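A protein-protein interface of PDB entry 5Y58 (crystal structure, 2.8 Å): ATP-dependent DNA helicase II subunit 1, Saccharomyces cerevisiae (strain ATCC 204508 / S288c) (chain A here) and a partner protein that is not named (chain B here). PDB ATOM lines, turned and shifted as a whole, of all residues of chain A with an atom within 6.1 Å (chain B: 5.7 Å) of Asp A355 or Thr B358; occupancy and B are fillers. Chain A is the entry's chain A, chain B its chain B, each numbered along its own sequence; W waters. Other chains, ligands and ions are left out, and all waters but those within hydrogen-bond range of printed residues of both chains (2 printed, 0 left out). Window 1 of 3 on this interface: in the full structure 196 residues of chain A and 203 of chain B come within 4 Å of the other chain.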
ATOM      1  N   TYR A 263      22.979 -27.688  -6.339  1.00  0.00           N
ATOM      2  CA  TYR A 263      24.377 -27.322  -6.151  1.00  0.00           C
ATOM      3  C   TYR A 263      25.258 -28.537  -5.887  1.00  0.00           C
ATOM      4  O   TYR A 263      25.223 -29.121  -4.805  1.00  0.00           O
ATOM      5  CB  TYR A 263      24.501 -26.306  -5.012  1.00  0.00           C
ATOM      6  CG  TYR A 263      23.732 -25.035  -5.293  1.00  0.00           C
ATOM      7  CD1 TYR A 263      24.242 -24.074  -6.154  1.00  0.00           C
ATOM      8  CD2 TYR A 263      22.482 -24.810  -4.723  1.00  0.00           C
ATOM      9  CE1 TYR A 263      23.539 -22.916  -6.426  1.00  0.00           C
ATOM     10  CE2 TYR A 263      21.773 -23.655  -4.994  1.00  0.00           C
ATOM     11  CZ  TYR A 263      22.307 -22.714  -5.848  1.00  0.00           C
ATOM     12  OH  TYR A 263      21.610 -21.561  -6.127  1.00  0.00           O
ATOM     13  N   THR A 264      26.038 -28.912  -6.897  1.00  0.00           N
ATOM     14  CA  THR A 264      26.980 -30.022  -6.796  1.00  0.00           C
ATOM     15  C   THR A 264      28.283 -29.585  -6.129  1.00  0.00           C
ATOM     16  O   THR A 264      28.428 -28.433  -5.716  1.00  0.00           O
ATOM     17  CB  THR A 264      27.306 -30.614  -8.181  1.00  0.00           C
ATOM     18  OG1 THR A 264      27.896 -29.605  -9.008  1.00  0.00           O
ATOM     19  CG2 THR A 264      26.045 -31.128  -8.853  1.00  0.00           C
ATOM     20  N   HIS A 265      29.228 -30.510  -6.019  1.00  0.00           N
ATOM     21  CA  HIS A 265      30.542 -30.190  -5.473  1.00  0.00           C
ATOM     22  C   HIS A 265      31.609 -30.622  -6.468  1.00  0.00           C
ATOM     23  O   HIS A 265      32.136 -31.730  -6.381  1.00  0.00           O
ATOM     24  CB  HIS A 265      30.759 -30.873  -4.121  1.00  0.00           C
ATOM     25  CG  HIS A 265      31.936 -30.352  -3.356  1.00  0.00           C
ATOM     26  ND1 HIS A 265      31.979 -30.324  -1.977  1.00  0.00           N
ATOM     27  CD2 HIS A 265      33.118 -29.838  -3.777  1.00  0.00           C
ATOM     28  CE1 HIS A 265      33.131 -29.818  -1.585  1.00  0.00           C
ATOM     29  NE2 HIS A 265      33.842 -29.512  -2.654  1.00  0.00           N
ATOM     30  N   ASN A 353      23.198 -27.806   8.940  1.00  0.00           N
ATOM     31  CA  ASN A 353      23.187 -28.457   7.635  1.00  0.00           C
ATOM     32  C   ASN A 353      24.150 -29.632   7.651  1.00  0.00           C
ATOM     33  O   ASN A 353      25.191 -29.577   8.299  1.00  0.00           O
ATOM     34  CB  ASN A 353      23.566 -27.485   6.520  1.00  0.00           C
ATOM     35  CG  ASN A 353      23.367 -28.083   5.138  1.00  0.00           C
ATOM     36  OD1 ASN A 353      22.296 -28.600   4.826  1.00  0.00           O
ATOM     37  ND2 ASN A 353      24.403 -28.029   4.310  1.00  0.00           N
ATOM     38  N   ILE A 354      23.793 -30.702   6.951  1.00  0.00           N
ATOM     39  CA  ILE A 354      24.613 -31.904   6.939  1.00  0.00           C
ATOM     40  C   ILE A 354      24.808 -32.414   5.519  1.00  0.00           C
ATOM     41  O   ILE A 354      25.709 -33.211   5.245  1.00  0.00           O
ATOM     42  CB  ILE A 354      23.987 -33.018   7.818  1.00  0.00           C
ATOM     43  CG1 ILE A 354      25.039 -34.062   8.197  1.00  0.00           C
ATOM     44  CG2 ILE A 354      22.780 -33.644   7.126  1.00  0.00           C
ATOM     45  CD1 ILE A 354      24.550 -35.072   9.194  1.00  0.00           C
ATOM     46  N   ASP A 355      23.974 -31.925   4.610  1.00  0.00           N
ATOM     47  CA  ASP A 355      23.999 -32.400   3.234  1.00  0.00           C
ATOM     48  C   ASP A 355      23.663 -31.281   2.258  1.00  0.00           C
ATOM     49  O   ASP A 355      23.499 -30.123   2.655  1.00  0.00           O
ATOM     50  CB  ASP A 355      23.015 -33.565   3.058  1.00  0.00           C
ATOM     51  CG  ASP A 355      23.509 -34.613   2.086  1.00  0.00           C
ATOM     52  OD1 ASP A 355      24.295 -34.260   1.184  1.00  0.00           O
ATOM     53  OD2 ASP A 355      23.118 -35.790   2.234  1.00  0.00           O
ATOM     54  N   LYS A 356      23.578 -31.635   0.980  1.00  0.00           N
ATOM     55  CA  LYS A 356      23.184 -30.697  -0.061  1.00  0.00           C
ATOM     56  C   LYS A 356      21.676 -30.758  -0.280  1.00  0.00           C
ATOM     57  O   LYS A 356      21.060 -31.812  -0.119  1.00  0.00           O
ATOM     58  CB  LYS A 356      23.937 -30.997  -1.362  1.00  0.00           C
ATOM     59  CG  LYS A 356      23.606 -32.350  -1.979  1.00  0.00           C
ATOM     60  CD  LYS A 356      24.518 -32.666  -3.147  1.00  0.00           C
ATOM     61  CE  LYS A 356      24.206 -34.047  -3.697  1.00  0.00           C
ATOM     62  NZ  LYS A 356      25.187 -34.461  -4.739  1.00  0.00           N
ATOM     63  N   SER A 357      21.092 -29.628  -0.658  1.00  0.00           N
ATOM     64  CA  SER A 357      19.653 -29.533  -0.856  1.00  0.00           C
ATOM     65  C   SER A 357      19.210 -30.024  -2.231  1.00  0.00           C
ATOM     66  O   SER A 357      19.959 -29.933  -3.206  1.00  0.00           O
ATOM     67  CB  SER A 357      19.209 -28.087  -0.650  1.00  0.00           C
ATOM     68  OG  SER A 357      20.136 -27.190  -1.254  1.00  0.00           O
ATOM     69  N   TYR A 403      13.658 -35.506   6.736  1.00  0.00           N
ATOM     70  CA  TYR A 403      13.907 -34.450   5.768  1.00  0.00           C
ATOM     71  C   TYR A 403      13.012 -33.256   6.039  1.00  0.00           C
ATOM     72  O   TYR A 403      11.924 -33.398   6.592  1.00  0.00           O
ATOM     73  CB  TYR A 403      13.696 -34.969   4.341  1.00  0.00           C
ATOM     74  CG  TYR A 403      14.810 -35.856   3.832  1.00  0.00           C
ATOM     75  CD1 TYR A 403      15.934 -35.311   3.224  1.00  0.00           C
ATOM     76  CD2 TYR A 403      14.736 -37.235   3.955  1.00  0.00           C
ATOM     77  CE1 TYR A 403      16.956 -36.117   2.759  1.00  0.00           C
ATOM     78  CE2 TYR A 403      15.756 -38.050   3.493  1.00  0.00           C
ATOM     79  CZ  TYR A 403      16.862 -37.484   2.894  1.00  0.00           C
ATOM     80  OH  TYR A 403      17.879 -38.288   2.431  1.00  0.00           O
ATOM     81  N   ARG A 421      18.147 -32.497   4.427  1.00  0.00           N
ATOM     82  CA  ARG A 421      18.236 -33.647   5.312  1.00  0.00           C
ATOM     83  C   ARG A 421      18.482 -33.200   6.745  1.00  0.00           C
ATOM     84  O   ARG A 421      19.289 -32.310   7.007  1.00  0.00           O
ATOM     85  CB  ARG A 421      19.333 -34.615   4.872  1.00  0.00           C
ATOM     86  CG  ARG A 421      19.236 -35.961   5.572  1.00  0.00           C
ATOM     87  CD  ARG A 421      20.172 -36.987   4.973  1.00  0.00           C
ATOM     88  NE  ARG A 421      21.512 -36.934   5.547  1.00  0.00           N
ATOM     89  CZ  ARG A 421      21.838 -37.446   6.731  1.00  0.00           C
ATOM     90  NH1 ARG A 421      23.084 -37.358   7.169  1.00  0.00           N
ATOM     91  NH2 ARG A 421      20.918 -38.037   7.483  1.00  0.00           N
ATOM     92  N   TYR B 355      19.224 -22.914   0.844  1.00  0.00           N
ATOM     93  CA  TYR B 355      19.689 -24.006  -0.002  1.00  0.00           C
ATOM     94  C   TYR B 355      21.121 -23.819  -0.509  1.00  0.00           C
ATOM     95  O   TYR B 355      21.640 -24.666  -1.238  1.00  0.00           O
ATOM     96  CB  TYR B 355      18.741 -24.186  -1.184  1.00  0.00           C
ATOM     97  CG  TYR B 355      18.345 -22.903  -1.885  1.00  0.00           C
ATOM     98  CD1 TYR B 355      19.180 -22.310  -2.824  1.00  0.00           C
ATOM     99  CD2 TYR B 355      17.119 -22.298  -1.626  1.00  0.00           C
ATOM    100  CE1 TYR B 355      18.811 -21.143  -3.474  1.00  0.00           C
ATOM    101  CE2 TYR B 355      16.743 -21.134  -2.268  1.00  0.00           C
ATOM    102  CZ  TYR B 355      17.589 -20.560  -3.191  1.00  0.00           C
ATOM    103  OH  TYR B 355      17.205 -19.399  -3.826  1.00  0.00           O
ATOM    104  N   PHE B 356      21.755 -22.715  -0.128  1.00  0.00           N
ATOM    105  CA  PHE B 356      23.140 -22.469  -0.507  1.00  0.00           C
ATOM    106  C   PHE B 356      24.097 -23.347   0.288  1.00  0.00           C
ATOM    107  O   PHE B 356      25.232 -23.568  -0.123  1.00  0.00           O
ATOM    108  CB  PHE B 356      23.496 -20.996  -0.310  1.00  0.00           C
ATOM    109  CG  PHE B 356      23.179 -20.129  -1.496  1.00  0.00           C
ATOM    110  CD1 PHE B 356      22.827 -20.694  -2.712  1.00  0.00           C
ATOM    111  CD2 PHE B 356      23.243 -18.745  -1.399  1.00  0.00           C
ATOM    112  CE1 PHE B 356      22.536 -19.898  -3.802  1.00  0.00           C
ATOM    113  CE2 PHE B 356      22.959 -17.948  -2.492  1.00  0.00           C
ATOM    114  CZ  PHE B 356      22.607 -18.525  -3.693  1.00  0.00           C
ATOM    115  N   LEU B 357      23.628 -23.847   1.426  1.00  0.00           N
ATOM    116  CA  LEU B 357      24.453 -24.654   2.321  1.00  0.00           C
ATOM    117  C   LEU B 357      24.598 -26.074   1.779  1.00  0.00           C
ATOM    118  O   LEU B 357      23.611 -26.801   1.681  1.00  0.00           O
ATOM    119  CB  LEU B 357      23.852 -24.678   3.729  1.00  0.00           C
ATOM    120  CG  LEU B 357      24.204 -23.559   4.719  1.00  0.00           C
ATOM    121  CD1 LEU B 357      24.102 -22.169   4.104  1.00  0.00           C
ATOM    122  CD2 LEU B 357      23.309 -23.666   5.944  1.00  0.00           C
ATOM    123  N   THR B 358      25.825 -26.466   1.439  1.00  0.00           N
ATOM    124  CA  THR B 358      26.058 -27.685   0.663  1.00  0.00           C
ATOM    125  C   THR B 358      26.801 -28.795   1.396  1.00  0.00           C
ATOM    126  O   THR B 358      26.900 -29.915   0.892  1.00  0.00           O
ATOM    127  CB  THR B 358      26.864 -27.379  -0.608  1.00  0.00           C
ATOM    128  OG1 THR B 358      28.176 -26.936  -0.243  1.00  0.00           O
ATOM    129  CG2 THR B 358      26.182 -26.305  -1.414  1.00  0.00           C
ATOM    130  N   SER B 359      27.335 -28.491   2.572  1.00  0.00           N
ATOM    131  CA  SER B 359      28.196 -29.444   3.257  1.00  0.00           C
ATOM    132  C   SER B 359      27.824 -29.684   4.710  1.00  0.00           C
ATOM    133  O   SER B 359      26.863 -29.117   5.224  1.00  0.00           O
ATOM    134  CB  SER B 359      29.645 -28.968   3.195  1.00  0.00           C
ATOM    135  OG  SER B 359      29.835 -27.881   4.086  1.00  0.00           O
ATOM    136  N   GLU B 360      28.606 -30.539   5.363  1.00  0.00           N
ATOM    137  CA  GLU B 360      28.474 -30.752   6.798  1.00  0.00           C
ATOM    138  C   GLU B 360      28.956 -29.500   7.521  1.00  0.00           C
ATOM    139  O   GLU B 360      29.722 -28.717   6.952  1.00  0.00           O
ATOM    140  CB  GLU B 360      29.272 -31.978   7.246  1.00  0.00           C
ATOM    141  CG  GLU B 360      28.858 -33.261   6.553  1.00  0.00           C
ATOM    142  CD  GLU B 360      29.700 -34.450   6.969  1.00  0.00           C
ATOM    143  OE1 GLU B 360      30.874 -34.253   7.353  1.00  0.00           O
ATOM    144  OE2 GLU B 360      29.182 -35.584   6.904  1.00  0.00           O
ATOM    145  N   CYS B 433      29.931 -23.658   7.233  1.00  0.00           N
ATOM    146  CA  CYS B 433      29.294 -24.518   6.242  1.00  0.00           C
ATOM    147  C   CYS B 433      29.557 -23.986   4.834  1.00  0.00           C
ATOM    148  O   CYS B 433      29.486 -22.782   4.599  1.00  0.00           O
ATOM    149  CB  CYS B 433      27.791 -24.624   6.504  1.00  0.00           C
ATOM    150  SG  CYS B 433      26.947 -25.831   5.461  1.00  0.00           S
ATOM    151  N   ARG B 434      29.853 -24.892   3.906  1.00  0.00           N
ATOM    152  CA  ARG B 434      30.334 -24.520   2.577  1.00  0.00           C
ATOM    153  C   ARG B 434      29.264 -23.906   1.680  1.00  0.00           C
ATOM    154  O   ARG B 434      28.132 -24.388   1.612  1.00  0.00           O
ATOM    155  CB  ARG B 434      30.939 -25.743   1.876  1.00  0.00           C
ATOM    156  CG  ARG B 434      31.509 -25.464   0.492  1.00  0.00           C
ATOM    157  CD  ARG B 434      32.027 -26.736  -0.154  1.00  0.00           C
ATOM    158  NE  ARG B 434      32.475 -26.510  -1.524  1.00  0.00           N
ATOM    159  CZ  ARG B 434      31.674 -26.560  -2.582  1.00  0.00           C
ATOM    160  NH1 ARG B 434      32.157 -26.342  -3.798  1.00  0.00           N
ATOM    161  NH2 ARG B 434      30.385 -26.825  -2.421  1.00  0.00           N
ATOM    162  N   LEU B 435      29.647 -22.838   0.986  1.00  0.00           N
ATOM    163  CA  LEU B 435      28.802 -22.211  -0.023  1.00  0.00           C
ATOM    164  C   LEU B 435      29.276 -22.648  -1.413  1.00  0.00           C
ATOM    165  O   LEU B 435      30.421 -23.066  -1.568  1.00  0.00           O
ATOM    166  CB  LEU B 435      28.841 -20.686   0.125  1.00  0.00           C
ATOM    167  CG  LEU B 435      28.231 -20.096   1.397  1.00  0.00           C
ATOM    168  CD1 LEU B 435      28.609 -18.628   1.558  1.00  0.00           C
ATOM    169  CD2 LEU B 435      26.729 -20.256   1.366  1.00  0.00           C
ATOM    170  N   PRO B 436      28.398 -22.565  -2.428  1.00  0.00           N
ATOM    171  CA  PRO B 436      28.754 -23.085  -3.755  1.00  0.00           C
ATOM    172  C   PRO B 436      29.551 -22.114  -4.622  1.00  0.00           C
ATOM    173  O   PRO B 436      29.337 -20.904  -4.567  1.00  0.00           O
ATOM    174  CB  PRO B 436      27.387 -23.369  -4.401  1.00  0.00           C
ATOM    175  CG  PRO B 436      26.331 -22.869  -3.420  1.00  0.00           C
ATOM    176  CD  PRO B 436      27.034 -22.012  -2.414  1.00  0.00           C
HETATM  177  O   HOH W   1      27.434 -32.984   0.914  1.00  0.00           O
HETATM  178  O   HOH W   2      34.891 -26.509  -2.688  1.00  0.00           O
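NE of Arg B434 sits close to NE2 of His A265, at 3.5 Å. The side-chain amide nitrogen (ND2) of Asn A353 is in hydrogen-bond range of the side-chain sulfur (SG) of Cys B433, 3.6 Å away. O of Tyr B355 is in hydrogen-bond range of OG of Ser A357 (2.9 Å). ND2 of Asn A353 sits at hydrogen-bond distance from O of Ser B359, at 2.8 Å. The backbone carbonyl oxygen of Leu B357 lies within hydrogen-bond range of the side-chain amide nitrogen of Asn A353. O of Leu B357 lies close to O of Asp A355, at 3.5 Å.
The side-chain hydroxyl (OG1) of Thr B358 sits at hydrogen-bond distance from the guanidinium group (NH2) of Arg B434. The side-chain amide nitrogen (ND2) of Asn A353 lies within hydrogen-bond range of the backbone carbonyl oxygen (O) of Asp A355, at 2.8 Å. The backbone carbonyl oxygen of Ser B359 is in hydrogen-bond range of the side-chain sulfur of Cys B433, at 3.3 Å. N of Arg B434 sits at hydrogen-bond distance from OG of Ser B359, at 3.0 Å. OD2 of Asp A355 is in salt-bridge range of NE of Arg A421, at 3.9 Å.
Among the printed residues, merely in contact across the chains: Tyr A263 with Tyr B355 (3.6 Å), Tyr A263 with Phe B356 (3.0 Å), Tyr A263 with Thr B358 (3.97 Å), Tyr A263 with Pro B436 (3.6 Å), Asn A353 with Thr B358 (3.6 Å), Asn A353 with Glu B360 (3.8 Å), Ile A354 with Ser B359 (3.9 Å), Ile A354 with Glu B360 (3.4 Å), Asp A355 with Thr B358 (3.8 Å) and Lys A356 with Thr B358 (3.7 Å).
Asp A355 touches just these residues of chain B: Leu B357 (3.5 Å) and Thr B358 (3.8 Å). Printed residues of chain A within 4 Å of Thr B358: Tyr A263, Asn A353, Asp A355 and Lys A356. Of the printed residues of chain A, Glu B360 touches Asn A353 and Ile A354. Printed residues of chain B within 4 Å of His A265: Arg B434. Of the printed residues of chain B, Lys A356 touches Thr B358. Arg A421 touches none of the printed residues of chain B. Thr A264 touches none of the printed residues of chain B. The nearest printed residue of chain A that does not touch Leu B357 is Lys A356 (4.3 Å).
Printed residues of chain A that touch a printed residue of chain B: Tyr A263, His A265, Asn A353, Ile A354, Asp A355, Lys A356 and Ser A357. Among the printed residues, 16 pairs touch across the chains. Among the printed residues, no Asp or Glu carboxylate lies within 4 Å of a Lys or Arg side-chain nitrogen of the other chain.
Water W2 bridges NE of Arg B434 (2.7 Å) and NE2 of His A265 (3.2 Å). Water W1 lies within hydrogen-bond range of the backbone carbonyl oxygen (O) of Thr B358 and the side-chain carboxylate (OD1) of Asp A355.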
